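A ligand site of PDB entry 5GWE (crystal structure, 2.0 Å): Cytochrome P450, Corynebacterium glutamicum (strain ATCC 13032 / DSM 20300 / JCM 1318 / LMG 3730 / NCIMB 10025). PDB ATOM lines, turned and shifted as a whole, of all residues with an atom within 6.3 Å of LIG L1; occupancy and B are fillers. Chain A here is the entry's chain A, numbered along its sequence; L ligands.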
ATOM      1  N   GLN A  60      14.237 -19.389  -9.637  1.00  0.00           N
ATOM      2  CA  GLN A  60      13.198 -18.382  -9.512  1.00  0.00           C
ATOM      3  C   GLN A  60      12.597 -18.308  -8.101  1.00  0.00           C
ATOM      4  O   GLN A  60      11.616 -17.595  -7.879  1.00  0.00           O
ATOM      5  CB  GLN A  60      12.098 -18.611 -10.544  1.00  0.00           C
ATOM      6  CG  GLN A  60      12.548 -18.447 -12.006  1.00  0.00           C
ATOM      7  CD  GLN A  60      13.048 -17.041 -12.317  1.00  0.00           C
ATOM      8  OE1 GLN A  60      12.508 -16.045 -11.818  1.00  0.00           O
ATOM      9  NE2 GLN A  60      14.104 -16.959 -13.119  1.00  0.00           N
ATOM     10  N   TYR A  82       5.325 -19.320 -11.538  1.00  0.00           N
ATOM     11  CA  TYR A  82       6.642 -19.530 -10.916  1.00  0.00           C
ATOM     12  C   TYR A  82       7.746 -19.301 -11.961  1.00  0.00           C
ATOM     13  O   TYR A  82       8.557 -18.369 -11.833  1.00  0.00           O
ATOM     14  CB  TYR A  82       6.762 -20.946 -10.318  1.00  0.00           C
ATOM     15  CG  TYR A  82       8.115 -21.180  -9.673  1.00  0.00           C
ATOM     16  CD1 TYR A  82       8.499 -20.445  -8.546  1.00  0.00           C
ATOM     17  CD2 TYR A  82       9.013 -22.100 -10.201  1.00  0.00           C
ATOM     18  CE1 TYR A  82       9.777 -20.638  -7.937  1.00  0.00           C
ATOM     19  CE2 TYR A  82      10.305 -22.284  -9.619  1.00  0.00           C
ATOM     20  CZ  TYR A  82      10.664 -21.553  -8.473  1.00  0.00           C
ATOM     21  OH  TYR A  82      11.903 -21.717  -7.865  1.00  0.00           O
ATOM     22  N   SER A  83       7.731 -20.118 -13.015  1.00  0.00           N
ATOM     23  CA  SER A  83       8.737 -19.983 -14.077  1.00  0.00           C
ATOM     24  C   SER A  83       8.225 -20.460 -15.442  1.00  0.00           C
ATOM     25  O   SER A  83       7.737 -21.580 -15.563  1.00  0.00           O
ATOM     26  CB  SER A  83       9.983 -20.783 -13.707  1.00  0.00           C
ATOM     27  OG  SER A  83      10.936 -20.669 -14.732  1.00  0.00           O
ATOM     28  N   GLY A  84       8.344 -19.618 -16.460  1.00  0.00           N
ATOM     29  CA  GLY A  84       7.993 -20.015 -17.815  1.00  0.00           C
ATOM     30  C   GLY A  84       8.926 -21.117 -18.297  1.00  0.00           C
ATOM     31  O   GLY A  84       8.481 -22.109 -18.879  1.00  0.00           O
ATOM     32  N   LEU A  85      10.230 -20.915 -18.088  1.00  0.00           N
ATOM     33  CA  LEU A  85      11.205 -21.897 -18.530  1.00  0.00           C
ATOM     34  C   LEU A  85      12.383 -22.067 -17.568  1.00  0.00           C
ATOM     35  O   LEU A  85      12.827 -23.185 -17.354  1.00  0.00           O
ATOM     36  CB  LEU A  85      11.777 -21.527 -19.899  1.00  0.00           C
ATOM     37  CG  LEU A  85      10.954 -21.949 -21.109  1.00  0.00           C
ATOM     38  CD1 LEU A  85      11.630 -21.432 -22.373  1.00  0.00           C
ATOM     39  CD2 LEU A  85      10.806 -23.504 -21.141  1.00  0.00           C
ATOM     40  N   SER A  86      12.931 -20.967 -17.049  1.00  0.00           N
ATOM     41  CA  SER A  86      14.303 -21.016 -16.474  1.00  0.00           C
ATOM     42  C   SER A  86      14.431 -21.946 -15.271  1.00  0.00           C
ATOM     43  O   SER A  86      15.517 -22.476 -15.041  1.00  0.00           O
ATOM     44  CB  SER A  86      14.812 -19.612 -16.087  1.00  0.00           C
ATOM     45  OG  SER A  86      14.285 -19.117 -14.852  1.00  0.00           O
ATOM     46  N   ALA A  87      13.360 -22.119 -14.515  1.00  0.00           N
ATOM     47  CA  ALA A  87      13.420 -22.937 -13.332  1.00  0.00           C
ATOM     48  C   ALA A  87      12.608 -24.227 -13.463  1.00  0.00           C
ATOM     49  O   ALA A  87      12.383 -24.918 -12.478  1.00  0.00           O
ATOM     50  CB  ALA A  87      12.956 -22.137 -12.090  1.00  0.00           C
ATOM     51  N   ARG A 171       9.568  -7.828 -10.298  1.00  0.00           N
ATOM     52  CA  ARG A 171       9.992  -9.235 -10.326  1.00  0.00           C
ATOM     53  C   ARG A 171      11.459  -9.358  -9.940  1.00  0.00           C
ATOM     54  O   ARG A 171      11.849 -10.232  -9.138  1.00  0.00           O
ATOM     55  CB  ARG A 171       9.728  -9.864 -11.696  1.00  0.00           C
ATOM     56  CG  ARG A 171      10.140 -11.342 -11.732  1.00  0.00           C
ATOM     57  CD  ARG A 171       9.603 -12.119 -12.948  1.00  0.00           C
ATOM     58  NE  ARG A 171      10.044 -13.532 -12.881  1.00  0.00           N
ATOM     59  CZ  ARG A 171       9.894 -14.425 -13.868  1.00  0.00           C
ATOM     60  NH1 ARG A 171       9.325 -14.073 -15.027  1.00  0.00           N
ATOM     61  NH2 ARG A 171      10.334 -15.675 -13.705  1.00  0.00           N
ATOM     62  N   TRP A 176      15.226 -11.461  -6.396  1.00  0.00           N
ATOM     63  CA  TRP A 176      16.686 -11.431  -6.134  1.00  0.00           C
ATOM     64  C   TRP A 176      17.118 -10.239  -5.271  1.00  0.00           C
ATOM     65  O   TRP A 176      18.307 -10.034  -5.066  1.00  0.00           O
ATOM     66  CB  TRP A 176      17.497 -11.386  -7.443  1.00  0.00           C
ATOM     67  CG  TRP A 176      17.294 -12.594  -8.347  1.00  0.00           C
ATOM     68  CD1 TRP A 176      18.000 -13.775  -8.344  1.00  0.00           C
ATOM     69  CD2 TRP A 176      16.286 -12.731  -9.353  1.00  0.00           C
ATOM     70  NE1 TRP A 176      17.514 -14.620  -9.312  1.00  0.00           N
ATOM     71  CE2 TRP A 176      16.449 -14.007  -9.934  1.00  0.00           C
ATOM     72  CE3 TRP A 176      15.255 -11.885  -9.809  1.00  0.00           C
ATOM     73  CZ2 TRP A 176      15.629 -14.463 -10.963  1.00  0.00           C
ATOM     74  CZ3 TRP A 176      14.442 -12.336 -10.833  1.00  0.00           C
ATOM     75  CH2 TRP A 176      14.622 -13.624 -11.391  1.00  0.00           C
ATOM     76  N   SER A 234       2.595 -18.609 -18.641  1.00  0.00           N
ATOM     77  CA  SER A 234       3.886 -18.644 -17.975  1.00  0.00           C
ATOM     78  C   SER A 234       5.038 -18.305 -18.940  1.00  0.00           C
ATOM     79  O   SER A 234       6.016 -17.653 -18.536  1.00  0.00           O
ATOM     80  CB  SER A 234       4.115 -20.019 -17.317  1.00  0.00           C
ATOM     81  OG  SER A 234       3.183 -20.213 -16.243  1.00  0.00           O
ATOM     82  N   TYR A 237       4.909 -14.638 -19.008  1.00  0.00           N
ATOM     83  CA  TYR A 237       5.517 -14.162 -17.748  1.00  0.00           C
ATOM     84  C   TYR A 237       7.050 -14.186 -17.892  1.00  0.00           C
ATOM     85  O   TYR A 237       7.758 -13.260 -17.483  1.00  0.00           O
ATOM     86  CB  TYR A 237       5.035 -15.047 -16.597  1.00  0.00           C
ATOM     87  CG  TYR A 237       5.580 -14.770 -15.211  1.00  0.00           C
ATOM     88  CD1 TYR A 237       5.266 -13.588 -14.526  1.00  0.00           C
ATOM     89  CD2 TYR A 237       6.371 -15.710 -14.554  1.00  0.00           C
ATOM     90  CE1 TYR A 237       5.768 -13.349 -13.241  1.00  0.00           C
ATOM     91  CE2 TYR A 237       6.847 -15.492 -13.273  1.00  0.00           C
ATOM     92  CZ  TYR A 237       6.549 -14.304 -12.638  1.00  0.00           C
ATOM     93  OH  TYR A 237       7.041 -14.109 -11.383  1.00  0.00           O
ATOM     94  N   SER A 238       7.560 -15.224 -18.530  1.00  0.00           N
ATOM     95  CA  SER A 238       8.996 -15.332 -18.798  1.00  0.00           C
ATOM     96  C   SER A 238       9.502 -14.275 -19.801  1.00  0.00           C
ATOM     97  O   SER A 238      10.348 -13.429 -19.482  1.00  0.00           O
ATOM     98  CB  SER A 238       9.308 -16.727 -19.318  1.00  0.00           C
ATOM     99  OG  SER A 238      10.664 -16.866 -19.697  1.00  0.00           O
ATOM    100  N   LEU A 239       8.946 -14.308 -21.002  1.00  0.00           N
ATOM    101  CA  LEU A 239       9.467 -13.468 -22.079  1.00  0.00           C
ATOM    102  C   LEU A 239       9.252 -11.973 -21.842  1.00  0.00           C
ATOM    103  O   LEU A 239      10.097 -11.162 -22.206  1.00  0.00           O
ATOM    104  CB  LEU A 239       8.819 -13.891 -23.377  1.00  0.00           C
ATOM    105  CG  LEU A 239       9.167 -15.327 -23.801  1.00  0.00           C
ATOM    106  CD1 LEU A 239       8.388 -15.694 -25.078  1.00  0.00           C
ATOM    107  CD2 LEU A 239      10.668 -15.541 -23.968  1.00  0.00           C
ATOM    108  N   PHE A 241       9.619 -10.439 -19.264  1.00  0.00           N
ATOM    109  CA  PHE A 241      10.581 -10.013 -18.250  1.00  0.00           C
ATOM    110  C   PHE A 241      12.009 -10.241 -18.751  1.00  0.00           C
ATOM    111  O   PHE A 241      12.780  -9.286 -18.935  1.00  0.00           O
ATOM    112  CB  PHE A 241      10.357 -10.780 -16.930  1.00  0.00           C
ATOM    113  CG  PHE A 241      11.436 -10.558 -15.900  1.00  0.00           C
ATOM    114  CD1 PHE A 241      11.581  -9.301 -15.262  1.00  0.00           C
ATOM    115  CD2 PHE A 241      12.290 -11.588 -15.549  1.00  0.00           C
ATOM    116  CE1 PHE A 241      12.573  -9.107 -14.313  1.00  0.00           C
ATOM    117  CE2 PHE A 241      13.277 -11.407 -14.603  1.00  0.00           C
ATOM    118  CZ  PHE A 241      13.431 -10.159 -13.971  1.00  0.00           C
ATOM    119  N   ALA A 242      12.327 -11.508 -19.002  1.00  0.00           N
ATOM    120  CA  ALA A 242      13.655 -11.879 -19.498  1.00  0.00           C
ATOM    121  C   ALA A 242      13.942 -11.249 -20.849  1.00  0.00           C
ATOM    122  O   ALA A 242      15.105 -11.087 -21.222  1.00  0.00           O
ATOM    123  CB  ALA A 242      13.785 -13.406 -19.599  1.00  0.00           C
ATOM    124  N   THR A 246      17.334  -7.470 -19.137  1.00  0.00           N
ATOM    125  CA  THR A 246      18.763  -7.658 -19.314  1.00  0.00           C
ATOM    126  C   THR A 246      19.315  -6.995 -20.599  1.00  0.00           C
ATOM    127  O   THR A 246      20.506  -6.751 -20.702  1.00  0.00           O
ATOM    128  CB  THR A 246      19.082  -9.139 -19.363  1.00  0.00           C
ATOM    129  OG1 THR A 246      18.163  -9.755 -20.278  1.00  0.00           O
ATOM    130  CG2 THR A 246      18.916  -9.782 -17.969  1.00  0.00           C
ATOM    131  N   ILE A 289      23.717 -10.251 -15.999  1.00  0.00           N
ATOM    132  CA  ILE A 289      23.524 -11.166 -14.851  1.00  0.00           C
ATOM    133  C   ILE A 289      24.902 -11.654 -14.406  1.00  0.00           C
ATOM    134  O   ILE A 289      25.670 -12.133 -15.232  1.00  0.00           O
ATOM    135  CB  ILE A 289      22.613 -12.364 -15.238  1.00  0.00           C
ATOM    136  CG1 ILE A 289      21.181 -11.847 -15.563  1.00  0.00           C
ATOM    137  CG2 ILE A 289      22.575 -13.434 -14.109  1.00  0.00           C
ATOM    138  CD1 ILE A 289      20.210 -12.966 -16.037  1.00  0.00           C
ATOM    139  N   TRP A 292      23.763 -16.852 -11.028  1.00  0.00           N
ATOM    140  CA  TRP A 292      22.538 -17.603 -11.296  1.00  0.00           C
ATOM    141  C   TRP A 292      22.537 -18.865 -10.453  1.00  0.00           C
ATOM    142  O   TRP A 292      23.607 -19.407 -10.150  1.00  0.00           O
ATOM    143  CB  TRP A 292      22.442 -17.932 -12.794  1.00  0.00           C
ATOM    144  CG  TRP A 292      21.028 -18.120 -13.302  1.00  0.00           C
ATOM    145  CD1 TRP A 292      20.493 -19.247 -13.861  1.00  0.00           C
ATOM    146  CD2 TRP A 292      19.992 -17.131 -13.306  1.00  0.00           C
ATOM    147  NE1 TRP A 292      19.177 -19.021 -14.219  1.00  0.00           N
ATOM    148  CE2 TRP A 292      18.847 -17.730 -13.891  1.00  0.00           C
ATOM    149  CE3 TRP A 292      19.910 -15.795 -12.876  1.00  0.00           C
ATOM    150  CZ2 TRP A 292      17.640 -17.049 -14.032  1.00  0.00           C
ATOM    151  CZ3 TRP A 292      18.715 -15.126 -13.045  1.00  0.00           C
ATOM    152  CH2 TRP A 292      17.596 -15.745 -13.614  1.00  0.00           C
ATOM    153  N   PHE A 393      21.281  -9.499 -10.790  1.00  0.00           N
ATOM    154  CA  PHE A 393      21.235  -8.529 -11.892  1.00  0.00           C
ATOM    155  C   PHE A 393      22.084  -7.315 -11.581  1.00  0.00           C
ATOM    156  O   PHE A 393      21.947  -6.723 -10.521  1.00  0.00           O
ATOM    157  CB  PHE A 393      19.783  -8.097 -12.182  1.00  0.00           C
ATOM    158  CG  PHE A 393      18.920  -9.212 -12.705  1.00  0.00           C
ATOM    159  CD1 PHE A 393      18.247 -10.062 -11.822  1.00  0.00           C
ATOM    160  CD2 PHE A 393      18.792  -9.445 -14.069  1.00  0.00           C
ATOM    161  CE1 PHE A 393      17.443 -11.115 -12.305  1.00  0.00           C
ATOM    162  CE2 PHE A 393      17.990 -10.488 -14.562  1.00  0.00           C
ATOM    163  CZ  PHE A 393      17.330 -11.335 -13.683  1.00  0.00           C
HETATM  164  C1  LIG L   1      17.340 -14.836 -17.016  1.00  0.00           C
HETATM  165  C2  LIG L   1      15.871 -15.178 -16.867  1.00  0.00           C
HETATM  166  C3  LIG L   1      15.081 -14.527 -15.923  1.00  0.00           C
HETATM  167  C4  LIG L   1      13.746 -14.862 -15.807  1.00  0.00           C
HETATM  168  C5  LIG L   1      13.196 -15.820 -16.649  1.00  0.00           C
HETATM  169  C6  LIG L   1      13.990 -16.452 -17.614  1.00  0.00           C
HETATM  170  C7  LIG L   1      15.320 -16.117 -17.722  1.00  0.00           C
HETATM  171  O1  LIG L   1      11.835 -16.094 -16.561  1.00  0.00           O
HETATM  172  P1  LIG L   1      11.228 -17.537 -16.295  1.00  0.00           P
HETATM  173  O2  LIG L   1      11.922 -18.189 -15.079  1.00  0.00           O
HETATM  174  O3  LIG L   1      11.480 -18.354 -17.617  1.00  0.00           O
HETATM  175  O4  LIG L   1       9.719 -17.292 -15.980  1.00  0.00           O
HETATM  176  C1  LG2 L   2      17.826 -17.917 -19.951  1.00  0.00           C
HETATM  177  C2  LG2 L   2      20.949 -14.233 -19.730  1.00  0.00           C
HETATM  178  C3  LG2 L   2      18.411 -11.732 -23.041  1.00  0.00           C
HETATM  179  C4  LG2 L   2      15.016 -15.195 -22.817  1.00  0.00           C
HETATM  180  C5  LG2 L   2      18.889 -17.120 -19.610  1.00  0.00           C
HETATM  181  C6  LG2 L   2      19.897 -17.443 -18.629  1.00  0.00           C
HETATM  182  C7  LG2 L   2      20.769 -16.435 -18.591  1.00  0.00           C
HETATM  183  C8  LG2 L   2      20.324 -15.436 -19.523  1.00  0.00           C
HETATM  184  C9  LG2 L   2      22.022 -16.343 -17.687  1.00  0.00           C
HETATM  185  C10 LG2 L   2      19.974 -18.745 -17.795  1.00  0.00           C
HETATM  186  C11 LG2 L   2      20.955 -19.661 -18.532  1.00  0.00           C
HETATM  187  C12 LG2 L   2      21.061 -21.027 -17.931  1.00  0.00           C
HETATM  188  O1  LG2 L   2      21.860 -21.874 -18.464  1.00  0.00           O
HETATM  189  O2  LG2 L   2      20.366 -21.281 -16.917  1.00  0.00           O
HETATM  190  C13 LG2 L   2      20.541 -13.248 -20.590  1.00  0.00           C
HETATM  191  C14 LG2 L   2      21.292 -12.032 -20.882  1.00  0.00           C
HETATM  192  C15 LG2 L   2      20.565 -11.356 -21.749  1.00  0.00           C
HETATM  193  C16 LG2 L   2      19.370 -12.100 -22.128  1.00  0.00           C
HETATM  194  C17 LG2 L   2      22.632 -11.506 -20.301  1.00  0.00           C
HETATM  195  C18 LG2 L   2      21.074 -10.034 -22.306  1.00  0.00           C
HETATM  196  C19 LG2 L   2      20.203  -9.209 -22.813  1.00  0.00           C
HETATM  197  C20 LG2 L   2      17.265 -12.471 -23.280  1.00  0.00           C
HETATM  198  C21 LG2 L   2      16.244 -12.121 -24.222  1.00  0.00           C
HETATM  199  C22 LG2 L   2      15.307 -13.100 -24.123  1.00  0.00           C
HETATM  200  C23 LG2 L   2      15.753 -14.082 -23.166  1.00  0.00           C
HETATM  201  C24 LG2 L   2      16.271 -10.840 -25.119  1.00  0.00           C
HETATM  202  C25 LG2 L   2      13.997 -13.307 -24.874  1.00  0.00           C
HETATM  203  C26 LG2 L   2      13.747 -12.739 -26.050  1.00  0.00           C
HETATM  204  C27 LG2 L   2      15.392 -16.231 -21.990  1.00  0.00           C
HETATM  205  C28 LG2 L   2      14.580 -17.378 -21.678  1.00  0.00           C
HETATM  206  C29 LG2 L   2      15.463 -18.225 -20.758  1.00  0.00           C
HETATM  207  C30 LG2 L   2      16.719 -17.510 -20.649  1.00  0.00           C
HETATM  208  C31 LG2 L   2      13.118 -17.661 -22.099  1.00  0.00           C
HETATM  209  C32 LG2 L   2      15.106 -19.563 -20.125  1.00  0.00           C
HETATM  210  C33 LG2 L   2      15.546 -20.635 -21.144  1.00  0.00           C
HETATM  211  C34 LG2 L   2      15.461 -22.026 -20.549  1.00  0.00           C
HETATM  212  O3  LG2 L   2      15.414 -23.022 -21.338  1.00  0.00           O
HETATM  213  O4  LG2 L   2      15.399 -22.167 -19.300  1.00  0.00           O
HETATM  214  N1  LG2 L   2      19.170 -15.885 -20.149  1.00  0.00           N
HETATM  215  N2  LG2 L   2      19.371 -13.242 -21.380  1.00  0.00           N
HETATM  216  N3  LG2 L   2      16.949 -13.680 -22.669  1.00  0.00           N
HETATM  217  N4  LG2 L   2      16.622 -16.367 -21.389  1.00  0.00           N
HETATM  218 FE1  LG2 L   2      18.162 -14.905 -21.629  1.00  0.00          FE
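The side-chain amide oxygen of Gln 60 lies within hydrogen-bond range of the guanidinium group of Arg 171 (2.9 Å).
NE2 of Gln 60 sits at hydrogen-bond distance from OG of Ser 86, 2.8 Å away.
The guanidinium group (NH1) of Arg 171 is in hydrogen-bond range of the backbone carbonyl oxygen (O) of Tyr 237 (3.0 Å).
OG of Ser 83 lies close to N of Leu 85 (3.4 Å).
The side-chain hydroxyl (OG) of Ser 83 lies within hydrogen-bond range of the backbone NH (N) of Ser 86.
O of Ala 242 sits at hydrogen-bond distance from OG1 of Thr 246 (3.5 Å).
The backbone NH (N) of Ala 87 sits at hydrogen-bond distance from the side-chain hydroxyl (OG) of Ser 83 (2.8 Å).
Residues that only touch LIG L1: Trp 292 (3.5 Å), Ile 289 (3.6 Å), Phe 241 (3.6 Å), Ala 242 (3.6 Å) and Tyr 237 (3.97 Å).
Hydrophobic or aromatic side chains that line LIG L1: Leu 85, Tyr 237, Phe 241, Ala 242, Ile 289 and Trp 292.
12 residues have an atom within 4 Å of LIG L1: Gln 60, Ser 83, Gly 84, Leu 85, Ser 86, Arg 171, Tyr 237, Ser 238, Phe 241, Ala 242, Ile 289 and Trp 292.
An oxygen (O2) of LIG L1 sits at hydrogen-bond distance from the side-chain hydroxyl (OG) of Ser 86, 2.5 Å away.
O3 of LIG L1 sits at hydrogen-bond distance from N of Ser 86.
O3 of LIG L1 is in hydrogen-bond range of OG of Ser 238, 2.7 Å away.
NH2 of Arg 171 is in salt-bridge range of O4 of LIG L1, 2.9 Å away.
OG of Ser 83 sits at hydrogen-bond distance from O2 of LIG L1, 2.7 Å away.
N of Leu 85 sits at hydrogen-bond distance from O3 of LIG L1.
NE2 of Gln 60 sits close to O2 of LIG L1 (3.2 Å).
The backbone NH of Gly 84 lies within hydrogen-bond range of an oxygen (O4) of LIG L1, at 2.7 Å.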
